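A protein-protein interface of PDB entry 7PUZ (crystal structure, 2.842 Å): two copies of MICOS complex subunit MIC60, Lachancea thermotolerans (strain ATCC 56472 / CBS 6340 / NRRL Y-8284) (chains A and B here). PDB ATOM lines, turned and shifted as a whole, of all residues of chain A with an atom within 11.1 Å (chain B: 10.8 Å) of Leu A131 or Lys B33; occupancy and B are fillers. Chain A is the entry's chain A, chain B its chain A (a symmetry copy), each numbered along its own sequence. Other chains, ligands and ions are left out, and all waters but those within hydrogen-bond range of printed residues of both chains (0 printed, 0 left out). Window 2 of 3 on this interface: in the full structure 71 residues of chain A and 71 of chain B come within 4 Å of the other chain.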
ATOM      1  N   LEU A 121     -15.402  31.927  18.995  1.00  0.00           N
ATOM      2  CA  LEU A 121     -16.287  30.798  19.276  1.00  0.00           C
ATOM      3  C   LEU A 121     -17.727  31.105  18.888  1.00  0.00           C
ATOM      4  O   LEU A 121     -18.428  30.250  18.331  1.00  0.00           O
ATOM      5  CB  LEU A 121     -16.207  30.424  20.754  1.00  0.00           C
ATOM      6  CG  LEU A 121     -14.879  29.807  21.199  1.00  0.00           C
ATOM      7  CD1 LEU A 121     -14.876  29.599  22.706  1.00  0.00           C
ATOM      8  CD2 LEU A 121     -14.628  28.498  20.469  1.00  0.00           C
ATOM      9  N   ALA A 122     -18.195  32.319  19.188  1.00  0.00           N
ATOM     10  CA  ALA A 122     -19.564  32.677  18.836  1.00  0.00           C
ATOM     11  C   ALA A 122     -19.759  32.670  17.327  1.00  0.00           C
ATOM     12  O   ALA A 122     -20.798  32.223  16.826  1.00  0.00           O
ATOM     13  CB  ALA A 122     -19.920  34.042  19.422  1.00  0.00           C
ATOM     14  N   GLU A 123     -18.759  33.147  16.582  1.00  0.00           N
ATOM     15  CA  GLU A 123     -18.829  33.076  15.128  1.00  0.00           C
ATOM     16  C   GLU A 123     -18.849  31.633  14.651  1.00  0.00           C
ATOM     17  O   GLU A 123     -19.537  31.306  13.679  1.00  0.00           O
ATOM     18  CB  GLU A 123     -17.653  33.820  14.504  1.00  0.00           C
ATOM     19  CG  GLU A 123     -17.786  35.320  14.513  1.00  0.00           C
ATOM     20  CD  GLU A 123     -16.570  35.993  13.909  1.00  0.00           C
ATOM     21  OE1 GLU A 123     -15.605  35.272  13.573  1.00  0.00           O
ATOM     22  OE2 GLU A 123     -16.580  37.235  13.772  1.00  0.00           O
ATOM     23  N   ALA A 124     -18.089  30.757  15.310  1.00  0.00           N
ATOM     24  CA  ALA A 124     -18.125  29.348  14.935  1.00  0.00           C
ATOM     25  C   ALA A 124     -19.513  28.759  15.154  1.00  0.00           C
ATOM     26  O   ALA A 124     -19.999  27.965  14.339  1.00  0.00           O
ATOM     27  CB  ALA A 124     -17.074  28.566  15.723  1.00  0.00           C
ATOM     28  N   VAL A 125     -20.169  29.149  16.245  1.00  0.00           N
ATOM     29  CA  VAL A 125     -21.542  28.709  16.486  1.00  0.00           C
ATOM     30  C   VAL A 125     -22.467  29.227  15.393  1.00  0.00           C
ATOM     31  O   VAL A 125     -23.337  28.501  14.898  1.00  0.00           O
ATOM     32  CB  VAL A 125     -22.011  29.166  17.876  1.00  0.00           C
ATOM     33  CG1 VAL A 125     -23.463  28.786  18.098  1.00  0.00           C
ATOM     34  CG2 VAL A 125     -21.122  28.569  18.937  1.00  0.00           C
ATOM     35  N   ASP A 126     -22.297  30.493  15.009  1.00  0.00           N
ATOM     36  CA  ASP A 126     -23.190  31.094  14.023  1.00  0.00           C
ATOM     37  C   ASP A 126     -22.952  30.542  12.619  1.00  0.00           C
ATOM     38  O   ASP A 126     -23.874  30.535  11.795  1.00  0.00           O
ATOM     39  CB  ASP A 126     -23.024  32.616  14.034  1.00  0.00           C
ATOM     40  CG  ASP A 126     -24.264  33.342  13.554  1.00  0.00           C
ATOM     41  OD1 ASP A 126     -25.361  33.041  14.069  1.00  0.00           O
ATOM     42  OD2 ASP A 126     -24.142  34.221  12.678  1.00  0.00           O
ATOM     43  N   GLN A 127     -21.737  30.073  12.331  1.00  0.00           N
ATOM     44  CA  GLN A 127     -21.355  29.609  11.001  1.00  0.00           C
ATOM     45  C   GLN A 127     -21.714  28.148  10.768  1.00  0.00           C
ATOM     46  O   GLN A 127     -22.293  27.801   9.735  1.00  0.00           O
ATOM     47  CB  GLN A 127     -19.849  29.803  10.789  1.00  0.00           C
ATOM     48  CG  GLN A 127     -19.465  30.954   9.871  1.00  0.00           C
ATOM     49  CD  GLN A 127     -19.621  32.310  10.530  1.00  0.00           C
ATOM     50  OE1 GLN A 127     -20.735  32.757  10.817  1.00  0.00           O
ATOM     51  NE2 GLN A 127     -18.496  32.969  10.789  1.00  0.00           N
ATOM     52  N   VAL A 128     -21.355  27.286  11.705  1.00  0.00           N
ATOM     53  CA  VAL A 128     -21.598  25.857  11.567  1.00  0.00           C
ATOM     54  C   VAL A 128     -23.032  25.553  11.976  1.00  0.00           C
ATOM     55  O   VAL A 128     -23.587  26.196  12.873  1.00  0.00           O
ATOM     56  CB  VAL A 128     -20.587  25.067  12.414  1.00  0.00           C
ATOM     57  CG1 VAL A 128     -20.829  23.569  12.296  1.00  0.00           C
ATOM     58  CG2 VAL A 128     -19.165  25.418  12.007  1.00  0.00           C
ATOM     59  N   ASP A 129     -23.648  24.585  11.300  1.00  0.00           N
ATOM     60  CA  ASP A 129     -25.004  24.152  11.608  1.00  0.00           C
ATOM     61  C   ASP A 129     -25.049  23.028  12.636  1.00  0.00           C
ATOM     62  O   ASP A 129     -26.142  22.594  13.013  1.00  0.00           O
ATOM     63  CB  ASP A 129     -25.721  23.703  10.326  1.00  0.00           C
ATOM     64  CG  ASP A 129     -25.949  24.847   9.346  1.00  0.00           C
ATOM     65  OD1 ASP A 129     -26.401  25.931   9.778  1.00  0.00           O
ATOM     66  OD2 ASP A 129     -25.679  24.660   8.142  1.00  0.00           O
ATOM     67  N   THR A 130     -23.902  22.540  13.090  1.00  0.00           N
ATOM     68  CA  THR A 130     -23.837  21.497  14.103  1.00  0.00           C
ATOM     69  C   THR A 130     -23.204  22.046  15.377  1.00  0.00           C
ATOM     70  O   THR A 130     -22.683  23.165  15.410  1.00  0.00           O
ATOM     71  CB  THR A 130     -23.051  20.285  13.589  1.00  0.00           C
ATOM     72  OG1 THR A 130     -21.702  20.678  13.307  1.00  0.00           O
ATOM     73  CG2 THR A 130     -23.688  19.741  12.321  1.00  0.00           C
ATOM     74  N   LEU A 131     -23.255  21.232  16.432  1.00  0.00           N
ATOM     75  CA  LEU A 131     -22.752  21.641  17.737  1.00  0.00           C
ATOM     76  C   LEU A 131     -21.279  22.029  17.659  1.00  0.00           C
ATOM     77  O   LEU A 131     -20.503  21.470  16.876  1.00  0.00           O
ATOM     78  CB  LEU A 131     -22.950  20.517  18.754  1.00  0.00           C
ATOM     79  CG  LEU A 131     -24.127  20.669  19.718  1.00  0.00           C
ATOM     80  CD1 LEU A 131     -25.382  21.116  18.990  1.00  0.00           C
ATOM     81  CD2 LEU A 131     -24.375  19.371  20.476  1.00  0.00           C
ATOM     82  N   VAL A 132     -20.896  23.001  18.487  1.00  0.00           N
ATOM     83  CA  VAL A 132     -19.549  23.562  18.450  1.00  0.00           C
ATOM     84  C   VAL A 132     -18.916  23.525  19.836  1.00  0.00           C
ATOM     85  O   VAL A 132     -17.704  23.319  19.968  1.00  0.00           O
ATOM     86  CB  VAL A 132     -19.571  24.994  17.880  1.00  0.00           C
ATOM     87  CG1 VAL A 132     -18.242  25.699  18.107  1.00  0.00           C
ATOM     88  CG2 VAL A 132     -19.896  24.965  16.391  1.00  0.00           C
ATOM     89  N   MET A 133     -19.721  23.707  20.882  1.00  0.00           N
ATOM     90  CA  MET A 133     -19.189  23.837  22.230  1.00  0.00           C
ATOM     91  C   MET A 133     -19.920  22.915  23.194  1.00  0.00           C
ATOM     92  O   MET A 133     -21.088  22.571  22.992  1.00  0.00           O
ATOM     93  CB  MET A 133     -19.291  25.277  22.741  1.00  0.00           C
ATOM     94  CG  MET A 133     -18.614  26.301  21.854  1.00  0.00           C
ATOM     95  SD  MET A 133     -19.296  27.926  22.191  1.00  0.00           S
ATOM     96  CE  MET A 133     -21.030  27.504  22.278  1.00  0.00           C
ATOM     97  N   LYS A 134     -19.211  22.539  24.256  1.00  0.00           N
ATOM     98  CA  LYS A 134     -19.799  21.773  25.349  1.00  0.00           C
ATOM     99  C   LYS A 134     -20.773  22.654  26.124  1.00  0.00           C
ATOM    100  O   LYS A 134     -20.374  23.682  26.681  1.00  0.00           O
ATOM    101  CB  LYS A 134     -18.694  21.251  26.266  1.00  0.00           C
ATOM    102  CG  LYS A 134     -17.457  20.763  25.521  1.00  0.00           C
ATOM    103  CD  LYS A 134     -16.264  20.573  26.449  1.00  0.00           C
ATOM    104  CE  LYS A 134     -15.023  20.141  25.672  1.00  0.00           C
ATOM    105  NZ  LYS A 134     -13.803  20.056  26.528  1.00  0.00           N
ATOM    106  N   SER A 135     -22.047  22.254  26.164  1.00  0.00           N
ATOM    107  CA  SER A 135     -23.070  23.106  26.763  1.00  0.00           C
ATOM    108  C   SER A 135     -22.865  23.263  28.267  1.00  0.00           C
ATOM    109  O   SER A 135     -23.206  24.306  28.835  1.00  0.00           O
ATOM    110  CB  SER A 135     -24.458  22.545  26.467  1.00  0.00           C
ATOM    111  OG  SER A 135     -24.588  21.248  27.016  1.00  0.00           O
ATOM    112  N   GLU A 136     -22.317  22.241  28.929  1.00  0.00           N
ATOM    113  CA  GLU A 136     -22.023  22.354  30.355  1.00  0.00           C
ATOM    114  C   GLU A 136     -21.001  23.456  30.611  1.00  0.00           C
ATOM    115  O   GLU A 136     -21.218  24.344  31.448  1.00  0.00           O
ATOM    116  CB  GLU A 136     -21.515  21.015  30.895  1.00  0.00           C
ATOM    117  CG  GLU A 136     -22.469  19.841  30.707  1.00  0.00           C
ATOM    118  CD  GLU A 136     -22.317  19.158  29.354  1.00  0.00           C
ATOM    119  OE1 GLU A 136     -21.364  19.491  28.614  1.00  0.00           O
ATOM    120  OE2 GLU A 136     -23.155  18.286  29.036  1.00  0.00           O
ATOM    121  N   LEU A 138     -20.260  25.854  28.621  1.00  0.00           N
ATOM    122  CA  LEU A 138     -20.815  27.135  28.187  1.00  0.00           C
ATOM    123  C   LEU A 138     -21.689  27.754  29.270  1.00  0.00           C
ATOM    124  O   LEU A 138     -21.583  28.951  29.560  1.00  0.00           O
ATOM    125  CB  LEU A 138     -21.609  26.954  26.895  1.00  0.00           C
ATOM    126  CG  LEU A 138     -22.230  28.237  26.355  1.00  0.00           C
ATOM    127  CD1 LEU A 138     -21.164  29.284  26.076  1.00  0.00           C
ATOM    128  CD2 LEU A 138     -23.020  27.928  25.100  1.00  0.00           C
ATOM    129  N   LEU A 176     -13.888  25.224  26.068  1.00  0.00           N
ATOM    130  CA  LEU A 176     -15.278  25.402  25.664  1.00  0.00           C
ATOM    131  C   LEU A 176     -15.613  24.652  24.373  1.00  0.00           C
ATOM    132  O   LEU A 176     -16.654  23.989  24.319  1.00  0.00           O
ATOM    133  CB  LEU A 176     -15.607  26.893  25.523  1.00  0.00           C
ATOM    134  CG  LEU A 176     -17.041  27.266  25.140  1.00  0.00           C
ATOM    135  CD1 LEU A 176     -18.033  26.512  26.000  1.00  0.00           C
ATOM    136  CD2 LEU A 176     -17.258  28.763  25.279  1.00  0.00           C
ATOM    137  N   PRO A 177     -14.793  24.731  23.317  1.00  0.00           N
ATOM    138  CA  PRO A 177     -15.161  24.031  22.077  1.00  0.00           C
ATOM    139  C   PRO A 177     -15.045  22.524  22.211  1.00  0.00           C
ATOM    140  O   PRO A 177     -14.255  22.001  23.003  1.00  0.00           O
ATOM    141  CB  PRO A 177     -14.150  24.575  21.059  1.00  0.00           C
ATOM    142  CG  PRO A 177     -12.977  24.949  21.874  1.00  0.00           C
ATOM    143  CD  PRO A 177     -13.547  25.500  23.144  1.00  0.00           C
ATOM    144  N   LEU A 178     -15.851  21.822  21.411  1.00  0.00           N
ATOM    145  CA  LEU A 178     -15.838  20.366  21.392  1.00  0.00           C
ATOM    146  C   LEU A 178     -14.501  19.836  20.891  1.00  0.00           C
ATOM    147  O   LEU A 178     -14.323  19.607  19.690  1.00  0.00           O
ATOM    148  CB  LEU A 178     -16.980  19.836  20.529  1.00  0.00           C
ATOM    149  CG  LEU A 178     -18.371  19.903  21.153  1.00  0.00           C
ATOM    150  CD1 LEU A 178     -19.439  19.473  20.165  1.00  0.00           C
ATOM    151  CD2 LEU A 178     -18.419  19.053  22.400  1.00  0.00           C
ATOM    152  N   GLU A 179     -13.566  19.630  21.814  1.00  0.00           N
ATOM    153  CA  GLU A 179     -12.233  19.116  21.506  1.00  0.00           C
ATOM    154  C   GLU A 179     -11.472  18.881  22.808  1.00  0.00           C
ATOM    155  O   GLU A 179     -10.997  17.779  23.080  1.00  0.00           O
ATOM    156  CB  GLU A 179     -11.453  20.083  20.604  1.00  0.00           C
ATOM    157  OXT GLU A 179     -11.323  19.794  23.625  1.00  0.00           O
ATOM    158  N   ILE B  30     -30.554  19.737  16.114  1.00  0.00           N
ATOM    159  CA  ILE B  30     -31.774  20.491  15.845  1.00  0.00           C
ATOM    160  C   ILE B  30     -32.099  21.416  17.016  1.00  0.00           C
ATOM    161  O   ILE B  30     -31.775  22.604  16.989  1.00  0.00           O
ATOM    162  CB  ILE B  30     -32.956  19.555  15.557  1.00  0.00           C
ATOM    163  N   ARG B  31     -32.747  20.860  18.045  1.00  0.00           N
ATOM    164  CA  ARG B  31     -33.023  21.626  19.257  1.00  0.00           C
ATOM    165  C   ARG B  31     -31.774  21.800  20.113  1.00  0.00           C
ATOM    166  O   ARG B  31     -31.652  22.803  20.828  1.00  0.00           O
ATOM    167  CB  ARG B  31     -34.135  20.952  20.065  1.00  0.00           C
ATOM    168  N   ALA B  32     -30.843  20.842  20.052  1.00  0.00           N
ATOM    169  CA  ALA B  32     -29.551  21.029  20.705  1.00  0.00           C
ATOM    170  C   ALA B  32     -28.812  22.226  20.116  1.00  0.00           C
ATOM    171  O   ALA B  32     -28.219  23.026  20.850  1.00  0.00           O
ATOM    172  CB  ALA B  32     -28.707  19.760  20.581  1.00  0.00           C
ATOM    173  N   LYS B  33     -28.851  22.378  18.788  1.00  0.00           N
ATOM    174  CA  LYS B  33     -28.203  23.523  18.155  1.00  0.00           C
ATOM    175  C   LYS B  33     -28.929  24.824  18.479  1.00  0.00           C
ATOM    176  O   LYS B  33     -28.290  25.867  18.663  1.00  0.00           O
ATOM    177  CB  LYS B  33     -28.126  23.316  16.642  1.00  0.00           C
ATOM    178  CG  LYS B  33     -27.300  24.362  15.929  1.00  0.00           C
ATOM    179  CD  LYS B  33     -25.921  24.468  16.552  1.00  0.00           C
ATOM    180  CE  LYS B  33     -25.174  25.690  16.042  1.00  0.00           C
ATOM    181  NZ  LYS B  33     -24.812  25.583  14.610  1.00  0.00           N
ATOM    182  N   SER B  34     -30.262  24.788  18.545  1.00  0.00           N
ATOM    183  CA  SER B  34     -31.016  25.977  18.924  1.00  0.00           C
ATOM    184  C   SER B  34     -30.659  26.417  20.339  1.00  0.00           C
ATOM    185  O   SER B  34     -30.459  27.612  20.600  1.00  0.00           O
ATOM    186  CB  SER B  34     -32.517  25.700  18.805  1.00  0.00           C
ATOM    187  OG  SER B  34     -33.284  26.891  18.862  1.00  0.00           O
ATOM    188  N   ARG B  35     -30.547  25.459  21.259  1.00  0.00           N
ATOM    189  CA  ARG B  35     -30.146  25.785  22.622  1.00  0.00           C
ATOM    190  C   ARG B  35     -28.711  26.293  22.668  1.00  0.00           C
ATOM    191  O   ARG B  35     -28.397  27.212  23.436  1.00  0.00           O
ATOM    192  CB  ARG B  35     -30.314  24.564  23.522  1.00  0.00           C
ATOM    193  CG  ARG B  35     -30.013  24.817  24.987  1.00  0.00           C
ATOM    194  CD  ARG B  35     -31.280  25.128  25.765  1.00  0.00           C
ATOM    195  NE  ARG B  35     -31.059  25.101  27.211  1.00  0.00           N
ATOM    196  CZ  ARG B  35     -31.059  26.180  27.987  1.00  0.00           C
ATOM    197  NH1 ARG B  35     -31.278  27.378  27.459  1.00  0.00           N
ATOM    198  NH2 ARG B  35     -30.853  26.062  29.291  1.00  0.00           N
ATOM    199  N   GLU B  36     -27.823  25.709  21.856  1.00  0.00           N
ATOM    200  CA  GLU B  36     -26.450  26.200  21.792  1.00  0.00           C
ATOM    201  C   GLU B  36     -26.410  27.649  21.331  1.00  0.00           C
ATOM    202  O   GLU B  36     -25.665  28.461  21.889  1.00  0.00           O
ATOM    203  CB  GLU B  36     -25.606  25.329  20.863  1.00  0.00           C
ATOM    204  CG  GLU B  36     -24.182  25.841  20.708  1.00  0.00           C
ATOM    205  CD  GLU B  36     -23.324  24.979  19.799  1.00  0.00           C
ATOM    206  OE1 GLU B  36     -23.436  25.116  18.563  1.00  0.00           O
ATOM    207  OE2 GLU B  36     -22.530  24.171  20.325  1.00  0.00           O
ATOM    208  N   VAL B  37     -27.204  27.992  20.317  1.00  0.00           N
ATOM    209  CA  VAL B  37     -27.237  29.366  19.824  1.00  0.00           C
ATOM    210  C   VAL B  37     -27.784  30.308  20.891  1.00  0.00           C
ATOM    211  O   VAL B  37     -27.238  31.397  21.119  1.00  0.00           O
ATOM    212  CB  VAL B  37     -28.052  29.442  18.518  1.00  0.00           C
ATOM    213  CG1 VAL B  37     -28.353  30.892  18.146  1.00  0.00           C
ATOM    214  CG2 VAL B  37     -27.305  28.730  17.391  1.00  0.00           C
ATOM    215  N   GLU B  38     -28.867  29.908  21.565  1.00  0.00           N
ATOM    216  CA  GLU B  38     -29.435  30.750  22.615  1.00  0.00           C
ATOM    217  C   GLU B  38     -28.416  31.003  23.724  1.00  0.00           C
ATOM    218  O   GLU B  38     -28.225  32.146  24.168  1.00  0.00           O
ATOM    219  CB  GLU B  38     -30.703  30.100  23.173  1.00  0.00           C
ATOM    220  CG  GLU B  38     -31.588  31.042  23.974  1.00  0.00           C
ATOM    221  CD  GLU B  38     -32.831  30.358  24.525  1.00  0.00           C
ATOM    222  OE1 GLU B  38     -33.010  29.144  24.271  1.00  0.00           O
ATOM    223  OE2 GLU B  38     -33.629  31.037  25.215  1.00  0.00           O
ATOM    224  N   LEU B  39     -27.730  29.947  24.167  1.00  0.00           N
ATOM    225  CA  LEU B  39     -26.751  30.095  25.240  1.00  0.00           C
ATOM    226  C   LEU B  39     -25.540  30.910  24.790  1.00  0.00           C
ATOM    227  O   LEU B  39     -24.993  31.697  25.571  1.00  0.00           O
ATOM    228  CB  LEU B  39     -26.317  28.721  25.746  1.00  0.00           C
ATOM    229  CG  LEU B  39     -27.303  27.880  26.551  1.00  0.00           C
ATOM    230  CD1 LEU B  39     -26.555  26.808  27.321  1.00  0.00           C
ATOM    231  CD2 LEU B  39     -28.123  28.751  27.488  1.00  0.00           C
ATOM    232  N   THR B  40     -25.095  30.725  23.543  1.00  0.00           N
ATOM    233  CA  THR B  40     -23.991  31.528  23.025  1.00  0.00           C
ATOM    234  C   THR B  40     -24.364  33.002  22.998  1.00  0.00           C
ATOM    235  O   THR B  40     -23.545  33.866  23.328  1.00  0.00           O
ATOM    236  CB  THR B  40     -23.604  31.045  21.625  1.00  0.00           C
ATOM    237  OG1 THR B  40     -23.196  29.678  21.689  1.00  0.00           O
ATOM    238  CG2 THR B  40     -22.462  31.870  21.056  1.00  0.00           C
ATOM    239  N   GLN B  41     -25.605  33.303  22.621  1.00  0.00           N
ATOM    240  CA  GLN B  41     -26.072  34.682  22.618  1.00  0.00           C
ATOM    241  C   GLN B  41     -26.064  35.264  24.027  1.00  0.00           C
ATOM    242  O   GLN B  41     -25.585  36.388  24.255  1.00  0.00           O
ATOM    243  CB  GLN B  41     -27.470  34.727  22.011  1.00  0.00           C
ATOM    244  CG  GLN B  41     -27.768  35.955  21.204  1.00  0.00           C
ATOM    245  CD  GLN B  41     -29.100  35.867  20.497  1.00  0.00           C
ATOM    246  OE1 GLN B  41     -29.837  34.897  20.659  1.00  0.00           O
ATOM    247  NE2 GLN B  41     -29.416  36.880  19.703  1.00  0.00           N
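O of Val A125 is in hydrogen-bond range of NZ of Lys B33 (3.3 Å). NZ of Lys B33 sits at hydrogen-bond distance from O of Thr A130, at 3.3 Å. The backbone NH (N) of Val A132 lies within hydrogen-bond range of the side-chain carboxylate (OE2) of Glu B36. OE2 of Glu B36 lies within hydrogen-bond range of N of Met A133 (2.9 Å). The backbone carbonyl oxygen of Val A128 sits close to the side-chain amino group of Lys B33.
O of Val A132 is in hydrogen-bond range of N of Leu A178 (2.8 Å). O of Glu B36 sits at hydrogen-bond distance from OG1 of Thr B40 (2.8 Å).
No position is printed for both chains.
Of the 21 printed residues of chain A, 9 touch a printed residue of chain B. Printed residues of chain A that touch a printed residue of chain B: Ala A122, Val A125, Val A128, Asp A129, Thr A130, Leu A131, Val A132, Met A133 and Leu A138. Hydrophobic or aromatic side chains of chain A that line the printed part of chain B: Ala A122, Val A125, Leu A131, Val A132, Met A133 and Leu A138. Among the printed residues, 17 pairs touch across the chains. Among the printed residues, no Asp or Glu carboxylate lies within 4 Å of a Lys or Arg side-chain nitrogen of the other chain.
Of the printed residues of chain B, Ala A122 touches Thr B40 (3.7 Å). Of chain B, only Lys B33, Glu B36, Val B37 and Thr B40 come within 4 Å of Val A125. Of the printed residues of chain B, Val A128 touches Lys B33. Thr A130 touches just these residues of chain B: Lys B33 and Glu B36. Printed residues of chain B within 4 Å of Leu A131: Ala B32, Lys B33 and Glu B36. Val A132 touches just one residue of chain B: Glu B36 (2.7 Å). Of the printed residues of chain B, Met A133 touches Glu B36 (2.9 Å) and Thr B40 (3.1 Å). Pro A177 touches none of the printed residues of chain B. Glu A179 touches none of the printed residues of chain B. Arg B31 touches none of the printed residues of chain A. Of chain A, only Leu A131 comes within 4 Å of Ala B32. Of chain A, only Val A125 (3.3 Å), Val A128 (2.2 Å), Asp A129 (3.2 Å), Thr A130 (3.3 Å) and Leu A131 (3.7 Å) come within 4 Å of Lys B33. No residue of chain A comes within 4 Å of Ser B34. Printed residues of chain A within 4 Å of Leu B39: Leu A138. Of the printed residues of chain A, Thr B40 touches Ala A122 (3.7 Å), Val A125 (3.6 Å), Met A133 (3.1 Å) and Leu A138 (3.8 Å). The nearest residue of chain B that does not touch Leu A131 is Ile B30 (6.1 Å).
Among the printed residues, pairs that only touch across the chains: Met A133 with Thr B40, Asp A129 with Lys B33, Leu A138 with Leu B39, Val A125 with Thr B40, Leu A131 with Glu B36, Leu A131 with Lys B33, Val A125 with Glu B36, Ala A122 with Thr B40, Leu A131 with Ala B32, Thr A130 with Glu B36, Leu A138 with Thr B40 and Val A125 with Val B37.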
